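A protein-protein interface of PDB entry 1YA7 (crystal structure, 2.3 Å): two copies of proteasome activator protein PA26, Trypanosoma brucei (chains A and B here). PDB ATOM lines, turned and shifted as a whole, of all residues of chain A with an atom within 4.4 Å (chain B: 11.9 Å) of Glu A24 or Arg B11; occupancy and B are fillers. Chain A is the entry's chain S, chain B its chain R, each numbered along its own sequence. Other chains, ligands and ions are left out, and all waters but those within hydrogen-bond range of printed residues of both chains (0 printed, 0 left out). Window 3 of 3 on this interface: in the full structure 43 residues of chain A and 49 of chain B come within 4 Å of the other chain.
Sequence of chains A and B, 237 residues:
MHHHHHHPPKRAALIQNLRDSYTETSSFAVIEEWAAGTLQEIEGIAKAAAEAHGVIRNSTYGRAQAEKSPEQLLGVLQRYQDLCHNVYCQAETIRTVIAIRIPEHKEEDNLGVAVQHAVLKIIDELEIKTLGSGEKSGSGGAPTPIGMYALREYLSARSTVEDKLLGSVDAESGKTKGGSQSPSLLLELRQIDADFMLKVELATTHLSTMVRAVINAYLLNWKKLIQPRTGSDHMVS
Hydrophobic or aromatic side chains of chain A within 4 Å of the printed part of chain B: Phe A28, Leu A219 and Trp A222. Along chain A the printed residues that touch a printed residue of chain B span positions 24 to 222. Hydrophobic or aromatic side chains of chain B within 4 Å of the printed part of chain A: Leu B14 and Ile B15.
The side-chain hydroxyl (OG) of Ser A27 lies within hydrogen-bond range of the backbone carbonyl oxygen (O) of Glu A24 (3.3 Å). OH of Tyr A218 lies within hydrogen-bond range of OE1 of Glu A24 (2.4 Å).
No position is printed for both chains. Of the 7 pairs that touch across the chains among the printed residues, none has its exchanged pair printed and touching as well.
CD1 of Phe A28 touches NH1 of Arg B11, at 3.8 Å. Phe A28 touches Leu B14 (CE1 to CD1, 3.8 Å). CD1 of Leu A219 touches O of Arg B11 (3.97 Å). CD1 of Leu A219 touches CB of Leu B14, at 3.6 Å. Leu A219 touches Ile B15 (CB to CD1, 3.5 Å). Trp A222 touches Arg B11.
NH2 of Arg B11 lies within salt-bridge range of OE2 of Glu A24 (2.7 Å).
No residue of chain B comes within 4 Å of Thr A23. Glu A24 touches just one residue of chain B: Arg B11. No residue of chain B comes within 4 Å of Thr A25. Phe A28 touches just these residues of chain B: Arg B11 and Leu B14. Trp A222 touches just one residue of chain B: Arg B11 (3.5 Å). Of the printed residues of chain A, Arg B11 touches Glu A24 (2.7 Å), Phe A28 (3.8 Å), Leu A219 (3.97 Å) and Trp A222 (3.5 Å). Of the printed residues of chain A, Leu B14 touches Phe A28 (3.8 Å) and Leu A219 (3.6 Å). Of the printed residues of chain A, Ile B15 touches Leu A219 (3.5 Å).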
ATOM      1  N   THR A  23     -21.434 -20.086   6.576  1.00  0.00           N
ATOM      2  CA  THR A  23     -22.290 -19.524   5.529  1.00  0.00           C
ATOM      3  C   THR A  23     -21.988 -18.036   5.369  1.00  0.00           C
ATOM      4  O   THR A  23     -21.212 -17.478   6.134  1.00  0.00           O
ATOM      5  CB  THR A  23     -23.804 -19.653   5.903  1.00  0.00           C
ATOM      6  OG1 THR A  23     -24.078 -18.776   7.006  1.00  0.00           O
ATOM      7  CG2 THR A  23     -24.196 -21.074   6.422  1.00  0.00           C
ATOM      8  N   GLU A  24     -22.624 -17.396   4.389  1.00  0.00           N
ATOM      9  CA  GLU A  24     -22.470 -15.953   4.191  1.00  0.00           C
ATOM     10  C   GLU A  24     -22.897 -15.151   5.434  1.00  0.00           C
ATOM     11  O   GLU A  24     -22.346 -14.102   5.717  1.00  0.00           O
ATOM     12  CB  GLU A  24     -23.202 -15.476   2.932  1.00  0.00           C
ATOM     13  CG  GLU A  24     -22.729 -14.103   2.446  1.00  0.00           C
ATOM     14  CD  GLU A  24     -23.313 -12.906   3.214  1.00  0.00           C
ATOM     15  OE1 GLU A  24     -22.548 -11.983   3.508  1.00  0.00           O
ATOM     16  OE2 GLU A  24     -24.525 -12.879   3.513  1.00  0.00           O
ATOM     17  N   THR A  25     -23.859 -15.676   6.187  1.00  0.00           N
ATOM     18  CA  THR A  25     -24.253 -15.098   7.471  1.00  0.00           C
ATOM     19  C   THR A  25     -23.132 -15.072   8.541  1.00  0.00           C
ATOM     20  O   THR A  25     -23.033 -14.117   9.324  1.00  0.00           O
ATOM     21  CB  THR A  25     -25.504 -15.831   8.007  1.00  0.00           C
ATOM     22  OG1 THR A  25     -26.596 -15.621   7.098  1.00  0.00           O
ATOM     23  CG2 THR A  25     -25.985 -15.149   9.297  1.00  0.00           C
ATOM     24  N   SER A  26     -22.299 -16.108   8.580  1.00  0.00           N
ATOM     25  CA  SER A  26     -21.117 -16.131   9.477  1.00  0.00           C
ATOM     26  C   SER A  26     -20.133 -14.984   9.183  1.00  0.00           C
ATOM     27  O   SER A  26     -19.657 -14.320  10.098  1.00  0.00           O
ATOM     28  CB  SER A  26     -20.377 -17.476   9.385  1.00  0.00           C
ATOM     29  OG  SER A  26     -21.305 -18.566   9.460  1.00  0.00           O
ATOM     30  N   SER A  27     -19.808 -14.764   7.916  1.00  0.00           N
ATOM     31  CA  SER A  27     -18.851 -13.708   7.581  1.00  0.00           C
ATOM     32  C   SER A  27     -19.517 -12.318   7.636  1.00  0.00           C
ATOM     33  O   SER A  27     -18.883 -11.349   8.046  1.00  0.00           O
ATOM     34  CB  SER A  27     -18.172 -13.970   6.224  1.00  0.00           C
ATOM     35  OG  SER A  27     -19.105 -14.294   5.203  1.00  0.00           O
ATOM     36  N   PHE A  28     -20.787 -12.238   7.251  1.00  0.00           N
ATOM     37  CA  PHE A  28     -21.530 -10.980   7.393  1.00  0.00           C
ATOM     38  C   PHE A  28     -21.594 -10.520   8.865  1.00  0.00           C
ATOM     39  O   PHE A  28     -21.358  -9.326   9.177  1.00  0.00           O
ATOM     40  CB  PHE A  28     -22.935 -11.074   6.781  1.00  0.00           C
ATOM     41  CG  PHE A  28     -23.708  -9.767   6.837  1.00  0.00           C
ATOM     42  CD1 PHE A  28     -23.185  -8.598   6.243  1.00  0.00           C
ATOM     43  CD2 PHE A  28     -24.923  -9.686   7.518  1.00  0.00           C
ATOM     44  CE1 PHE A  28     -23.879  -7.373   6.288  1.00  0.00           C
ATOM     45  CE2 PHE A  28     -25.628  -8.458   7.587  1.00  0.00           C
ATOM     46  CZ  PHE A  28     -25.097  -7.292   6.957  1.00  0.00           C
ATOM     47  N   TYR A 218     -15.362  -6.516   1.422  1.00  0.00           N
ATOM     48  CA  TYR A 218     -16.347  -7.584   1.606  1.00  0.00           C
ATOM     49  C   TYR A 218     -17.712  -7.235   1.054  1.00  0.00           C
ATOM     50  O   TYR A 218     -18.304  -8.023   0.331  1.00  0.00           O
ATOM     51  CB  TYR A 218     -16.523  -7.977   3.081  1.00  0.00           C
ATOM     52  CG  TYR A 218     -17.503  -9.132   3.248  1.00  0.00           C
ATOM     53  CD1 TYR A 218     -17.064 -10.459   3.125  1.00  0.00           C
ATOM     54  CD2 TYR A 218     -18.861  -8.908   3.516  1.00  0.00           C
ATOM     55  CE1 TYR A 218     -17.949 -11.542   3.262  1.00  0.00           C
ATOM     56  CE2 TYR A 218     -19.746  -9.962   3.669  1.00  0.00           C
ATOM     57  CZ  TYR A 218     -19.289 -11.287   3.538  1.00  0.00           C
ATOM     58  OH  TYR A 218     -20.167 -12.369   3.680  1.00  0.00           O
ATOM     59  N   LEU A 219     -18.222  -6.067   1.424  1.00  0.00           N
ATOM     60  CA  LEU A 219     -19.595  -5.703   1.127  1.00  0.00           C
ATOM     61  C   LEU A 219     -19.776  -5.418  -0.356  1.00  0.00           C
ATOM     62  O   LEU A 219     -20.851  -5.625  -0.918  1.00  0.00           O
ATOM     63  CB  LEU A 219     -20.006  -4.483   1.962  1.00  0.00           C
ATOM     64  CG  LEU A 219     -20.090  -4.641   3.490  1.00  0.00           C
ATOM     65  CD1 LEU A 219     -20.366  -3.308   4.191  1.00  0.00           C
ATOM     66  CD2 LEU A 219     -21.118  -5.695   3.894  1.00  0.00           C
ATOM     67  N   TRP A 222     -19.199  -9.370  -2.003  1.00  0.00           N
ATOM     68  CA  TRP A 222     -19.660 -10.603  -1.307  1.00  0.00           C
ATOM     69  C   TRP A 222     -20.370 -11.650  -2.199  1.00  0.00           C
ATOM     70  O   TRP A 222     -20.228 -12.830  -1.973  1.00  0.00           O
ATOM     71  CB  TRP A 222     -20.519 -10.258  -0.084  1.00  0.00           C
ATOM     72  CG  TRP A 222     -21.901  -9.784  -0.430  1.00  0.00           C
ATOM     73  CD1 TRP A 222     -22.299  -8.489  -0.668  1.00  0.00           C
ATOM     74  CD2 TRP A 222     -23.075 -10.602  -0.595  1.00  0.00           C
ATOM     75  NE1 TRP A 222     -23.637  -8.459  -0.995  1.00  0.00           N
ATOM     76  CE2 TRP A 222     -24.147  -9.737  -0.931  1.00  0.00           C
ATOM     77  CE3 TRP A 222     -23.330 -11.986  -0.505  1.00  0.00           C
ATOM     78  CZ2 TRP A 222     -25.453 -10.212  -1.181  1.00  0.00           C
ATOM     79  CZ3 TRP A 222     -24.637 -12.461  -0.742  1.00  0.00           C
ATOM     80  CH2 TRP A 222     -25.679 -11.573  -1.072  1.00  0.00           C
ATOM     81  N   ILE A 226     -19.243 -15.801  -2.480  1.00  0.00           N
ATOM     82  CA  ILE A 226     -20.087 -16.969  -2.222  1.00  0.00           C
ATOM     83  C   ILE A 226     -20.387 -17.783  -3.487  1.00  0.00           C
ATOM     84  O   ILE A 226     -20.363 -19.016  -3.467  1.00  0.00           O
ATOM     85  CB  ILE A 226     -21.443 -16.522  -1.584  1.00  0.00           C
ATOM     86  CG1 ILE A 226     -21.192 -15.623  -0.364  1.00  0.00           C
ATOM     87  CG2 ILE A 226     -22.315 -17.755  -1.268  1.00  0.00           C
ATOM     88  CD1 ILE A 226     -20.355 -16.278   0.761  1.00  0.00           C
ATOM     89  N   LYS B  10     -28.212  -3.964   6.766  1.00  0.00           N
ATOM     90  CA  LYS B  10     -28.290  -3.475   5.344  1.00  0.00           C
ATOM     91  C   LYS B  10     -26.925  -2.984   4.812  1.00  0.00           C
ATOM     92  O   LYS B  10     -26.260  -2.132   5.410  1.00  0.00           O
ATOM     93  CB  LYS B  10     -29.360  -2.398   5.194  1.00  0.00           C
ATOM     94  CG  LYS B  10     -30.042  -2.294   3.819  1.00  0.00           C
ATOM     95  CD  LYS B  10     -31.421  -1.576   3.980  1.00  0.00           C
ATOM     96  CE  LYS B  10     -32.161  -1.417   2.655  1.00  0.00           C
ATOM     97  NZ  LYS B  10     -31.564  -0.367   1.758  1.00  0.00           N
ATOM     98  N   ARG B  11     -26.528  -3.549   3.677  1.00  0.00           N
ATOM     99  CA  ARG B  11     -25.151  -3.495   3.183  1.00  0.00           C
ATOM    100  C   ARG B  11     -24.780  -2.130   2.607  1.00  0.00           C
ATOM    101  O   ARG B  11     -23.713  -1.599   2.906  1.00  0.00           O
ATOM    102  CB  ARG B  11     -24.939  -4.619   2.161  1.00  0.00           C
ATOM    103  CG  ARG B  11     -25.166  -6.006   2.768  1.00  0.00           C
ATOM    104  CD  ARG B  11     -25.295  -7.124   1.772  1.00  0.00           C
ATOM    105  NE  ARG B  11     -25.792  -8.340   2.426  1.00  0.00           N
ATOM    106  CZ  ARG B  11     -25.031  -9.365   2.804  1.00  0.00           C
ATOM    107  NH1 ARG B  11     -23.717  -9.374   2.579  1.00  0.00           N
ATOM    108  NH2 ARG B  11     -25.596 -10.394   3.402  1.00  0.00           N
ATOM    109  N   ALA B  12     -25.680  -1.565   1.803  1.00  0.00           N
ATOM    110  CA  ALA B  12     -25.471  -0.241   1.222  1.00  0.00           C
ATOM    111  C   ALA B  12     -25.361   0.813   2.332  1.00  0.00           C
ATOM    112  O   ALA B  12     -24.531   1.727   2.246  1.00  0.00           O
ATOM    113  CB  ALA B  12     -26.570   0.102   0.209  1.00  0.00           C
ATOM    114  N   ALA B  13     -26.153   0.652   3.397  1.00  0.00           N
ATOM    115  CA  ALA B  13     -26.091   1.555   4.551  1.00  0.00           C
ATOM    116  C   ALA B  13     -24.775   1.406   5.300  1.00  0.00           C
ATOM    117  O   ALA B  13     -24.200   2.399   5.756  1.00  0.00           O
ATOM    118  CB  ALA B  13     -27.258   1.318   5.472  1.00  0.00           C
ATOM    119  N   LEU B  14     -24.278   0.169   5.427  1.00  0.00           N
ATOM    120  CA  LEU B  14     -22.945  -0.014   6.018  1.00  0.00           C
ATOM    121  C   LEU B  14     -21.871   0.667   5.184  1.00  0.00           C
ATOM    122  O   LEU B  14     -21.003   1.313   5.750  1.00  0.00           O
ATOM    123  CB  LEU B  14     -22.621  -1.483   6.300  1.00  0.00           C
ATOM    124  CG  LEU B  14     -23.452  -2.149   7.421  1.00  0.00           C
ATOM    125  CD1 LEU B  14     -23.545  -3.678   7.252  1.00  0.00           C
ATOM    126  CD2 LEU B  14     -22.913  -1.782   8.798  1.00  0.00           C
ATOM    127  N   ILE B  15     -21.944   0.544   3.851  1.00  0.00           N
ATOM    128  CA  ILE B  15     -20.948   1.171   2.969  1.00  0.00           C
ATOM    129  C   ILE B  15     -21.002   2.688   3.115  1.00  0.00           C
ATOM    130  O   ILE B  15     -19.977   3.326   3.301  1.00  0.00           O
ATOM    131  CB  ILE B  15     -21.170   0.790   1.462  1.00  0.00           C
ATOM    132  CG1 ILE B  15     -20.870  -0.694   1.187  1.00  0.00           C
ATOM    133  CG2 ILE B  15     -20.286   1.669   0.550  1.00  0.00           C
ATOM    134  CD1 ILE B  15     -19.460  -1.054   1.472  1.00  0.00           C
ATOM    135  N   GLN B  16     -22.218   3.239   3.020  1.00  0.00           N
ATOM    136  CA  GLN B  16     -22.467   4.678   3.125  1.00  0.00           C
ATOM    137  C   GLN B  16     -22.016   5.250   4.464  1.00  0.00           C
ATOM    138  O   GLN B  16     -21.383   6.308   4.494  1.00  0.00           O
ATOM    139  CB  GLN B  16     -23.941   5.028   2.812  1.00  0.00           C
ATOM    140  CG  GLN B  16     -24.164   6.508   2.383  1.00  0.00           C
ATOM    141  CD  GLN B  16     -23.158   6.999   1.298  1.00  0.00           C
ATOM    142  OE1 GLN B  16     -22.786   6.232   0.382  1.00  0.00           O
ATOM    143  NE2 GLN B  16     -22.715   8.266   1.409  1.00  0.00           N
ATOM    144  N   ASN B  17     -22.287   4.535   5.564  1.00  0.00           N
ATOM    145  CA  ASN B  17     -21.786   4.971   6.888  1.00  0.00           C
ATOM    146  C   ASN B  17     -20.270   5.058   6.963  1.00  0.00           C
ATOM    147  O   ASN B  17     -19.726   5.979   7.574  1.00  0.00           O
ATOM    148  CB  ASN B  17     -22.307   4.089   8.025  1.00  0.00           C
ATOM    149  CG  ASN B  17     -21.767   4.531   9.402  1.00  0.00           C
ATOM    150  OD1 ASN B  17     -22.401   5.355  10.119  1.00  0.00           O
ATOM    151  ND2 ASN B  17     -20.577   4.021   9.766  1.00  0.00           N
ATOM    152  N   LEU B  18     -19.593   4.073   6.360  1.00  0.00           N
ATOM    153  CA  LEU B  18     -18.147   4.084   6.218  1.00  0.00           C
ATOM    154  C   LEU B  18     -17.696   5.294   5.457  1.00  0.00           C
ATOM    155  O   LEU B  18     -16.846   6.024   5.911  1.00  0.00           O
ATOM    156  CB  LEU B  18     -17.675   2.858   5.416  1.00  0.00           C
ATOM    157  CG  LEU B  18     -16.900   1.713   6.028  1.00  0.00           C
ATOM    158  CD1 LEU B  18     -16.067   1.057   4.912  1.00  0.00           C
ATOM    159  CD2 LEU B  18     -16.038   2.166   7.191  1.00  0.00           C
ATOM    160  N   ARG B  19     -18.247   5.492   4.271  1.00  0.00           N
ATOM    161  CA  ARG B  19     -17.802   6.594   3.407  1.00  0.00           C
ATOM    162  C   ARG B  19     -18.158   8.010   3.854  1.00  0.00           C
ATOM    163  O   ARG B  19     -17.438   8.946   3.529  1.00  0.00           O
ATOM    164  CB  ARG B  19     -18.240   6.362   1.952  1.00  0.00           C
ATOM    165  CG  ARG B  19     -17.578   5.136   1.341  1.00  0.00           C
ATOM    166  CD  ARG B  19     -17.966   4.890  -0.085  1.00  0.00           C
ATOM    167  NE  ARG B  19     -17.377   3.651  -0.596  1.00  0.00           N
ATOM    168  CZ  ARG B  19     -17.808   3.046  -1.693  1.00  0.00           C
ATOM    169  NH1 ARG B  19     -18.825   3.584  -2.379  1.00  0.00           N
ATOM    170  NH2 ARG B  19     -17.243   1.902  -2.104  1.00  0.00           N
ATOM    171  N   ASP B  20     -19.273   8.177   4.553  1.00  0.00           N
ATOM    172  CA  ASP B  20     -19.580   9.466   5.228  1.00  0.00           C
ATOM    173  C   ASP B  20     -18.571   9.815   6.319  1.00  0.00           C
ATOM    174  O   ASP B  20     -18.309  10.981   6.568  1.00  0.00           O
ATOM    175  CB  ASP B  20     -20.953   9.423   5.892  1.00  0.00           C
ATOM    176  CG  ASP B  20     -22.062   9.261   4.907  1.00  0.00           C
ATOM    177  OD1 ASP B  20     -21.824   9.443   3.689  1.00  0.00           O
ATOM    178  OD2 ASP B  20     -23.210   8.947   5.266  1.00  0.00           O
ATOM    179  N   ILE B 100     -11.483   2.918   1.414  1.00  0.00           N
ATOM    180  CA  ILE B 100     -12.894   2.591   1.561  1.00  0.00           C
ATOM    181  C   ILE B 100     -13.691   2.890   0.287  1.00  0.00           C
ATOM    182  O   ILE B 100     -14.921   2.736   0.260  1.00  0.00           O
ATOM    183  CB  ILE B 100     -13.526   3.294   2.820  1.00  0.00           C
ATOM    184  CG1 ILE B 100     -13.674   4.827   2.631  1.00  0.00           C
ATOM    185  CG2 ILE B 100     -12.749   2.942   4.054  1.00  0.00           C
ATOM    186  CD1 ILE B 100     -14.175   5.577   3.897  1.00  0.00           C
ATOM    187  N   GLU B 104     -15.808  -2.380  -6.512  1.00  0.00           N
ATOM    188  CA  GLU B 104     -15.976  -3.813  -6.796  1.00  0.00           C
ATOM    189  C   GLU B 104     -14.808  -4.322  -7.679  1.00  0.00           C
ATOM    190  O   GLU B 104     -14.442  -3.687  -8.693  1.00  0.00           O
ATOM    191  CB  GLU B 104     -17.292  -4.040  -7.526  1.00  0.00           C
ATOM    192  CG  GLU B 104     -17.637  -5.515  -7.747  1.00  0.00           C
ATOM    193  CD  GLU B 104     -18.871  -5.689  -8.623  1.00  0.00           C
ATOM    194  OE1 GLU B 104     -19.818  -4.907  -8.470  1.00  0.00           O
ATOM    195  OE2 GLU B 104     -18.900  -6.601  -9.482  1.00  0.00           O
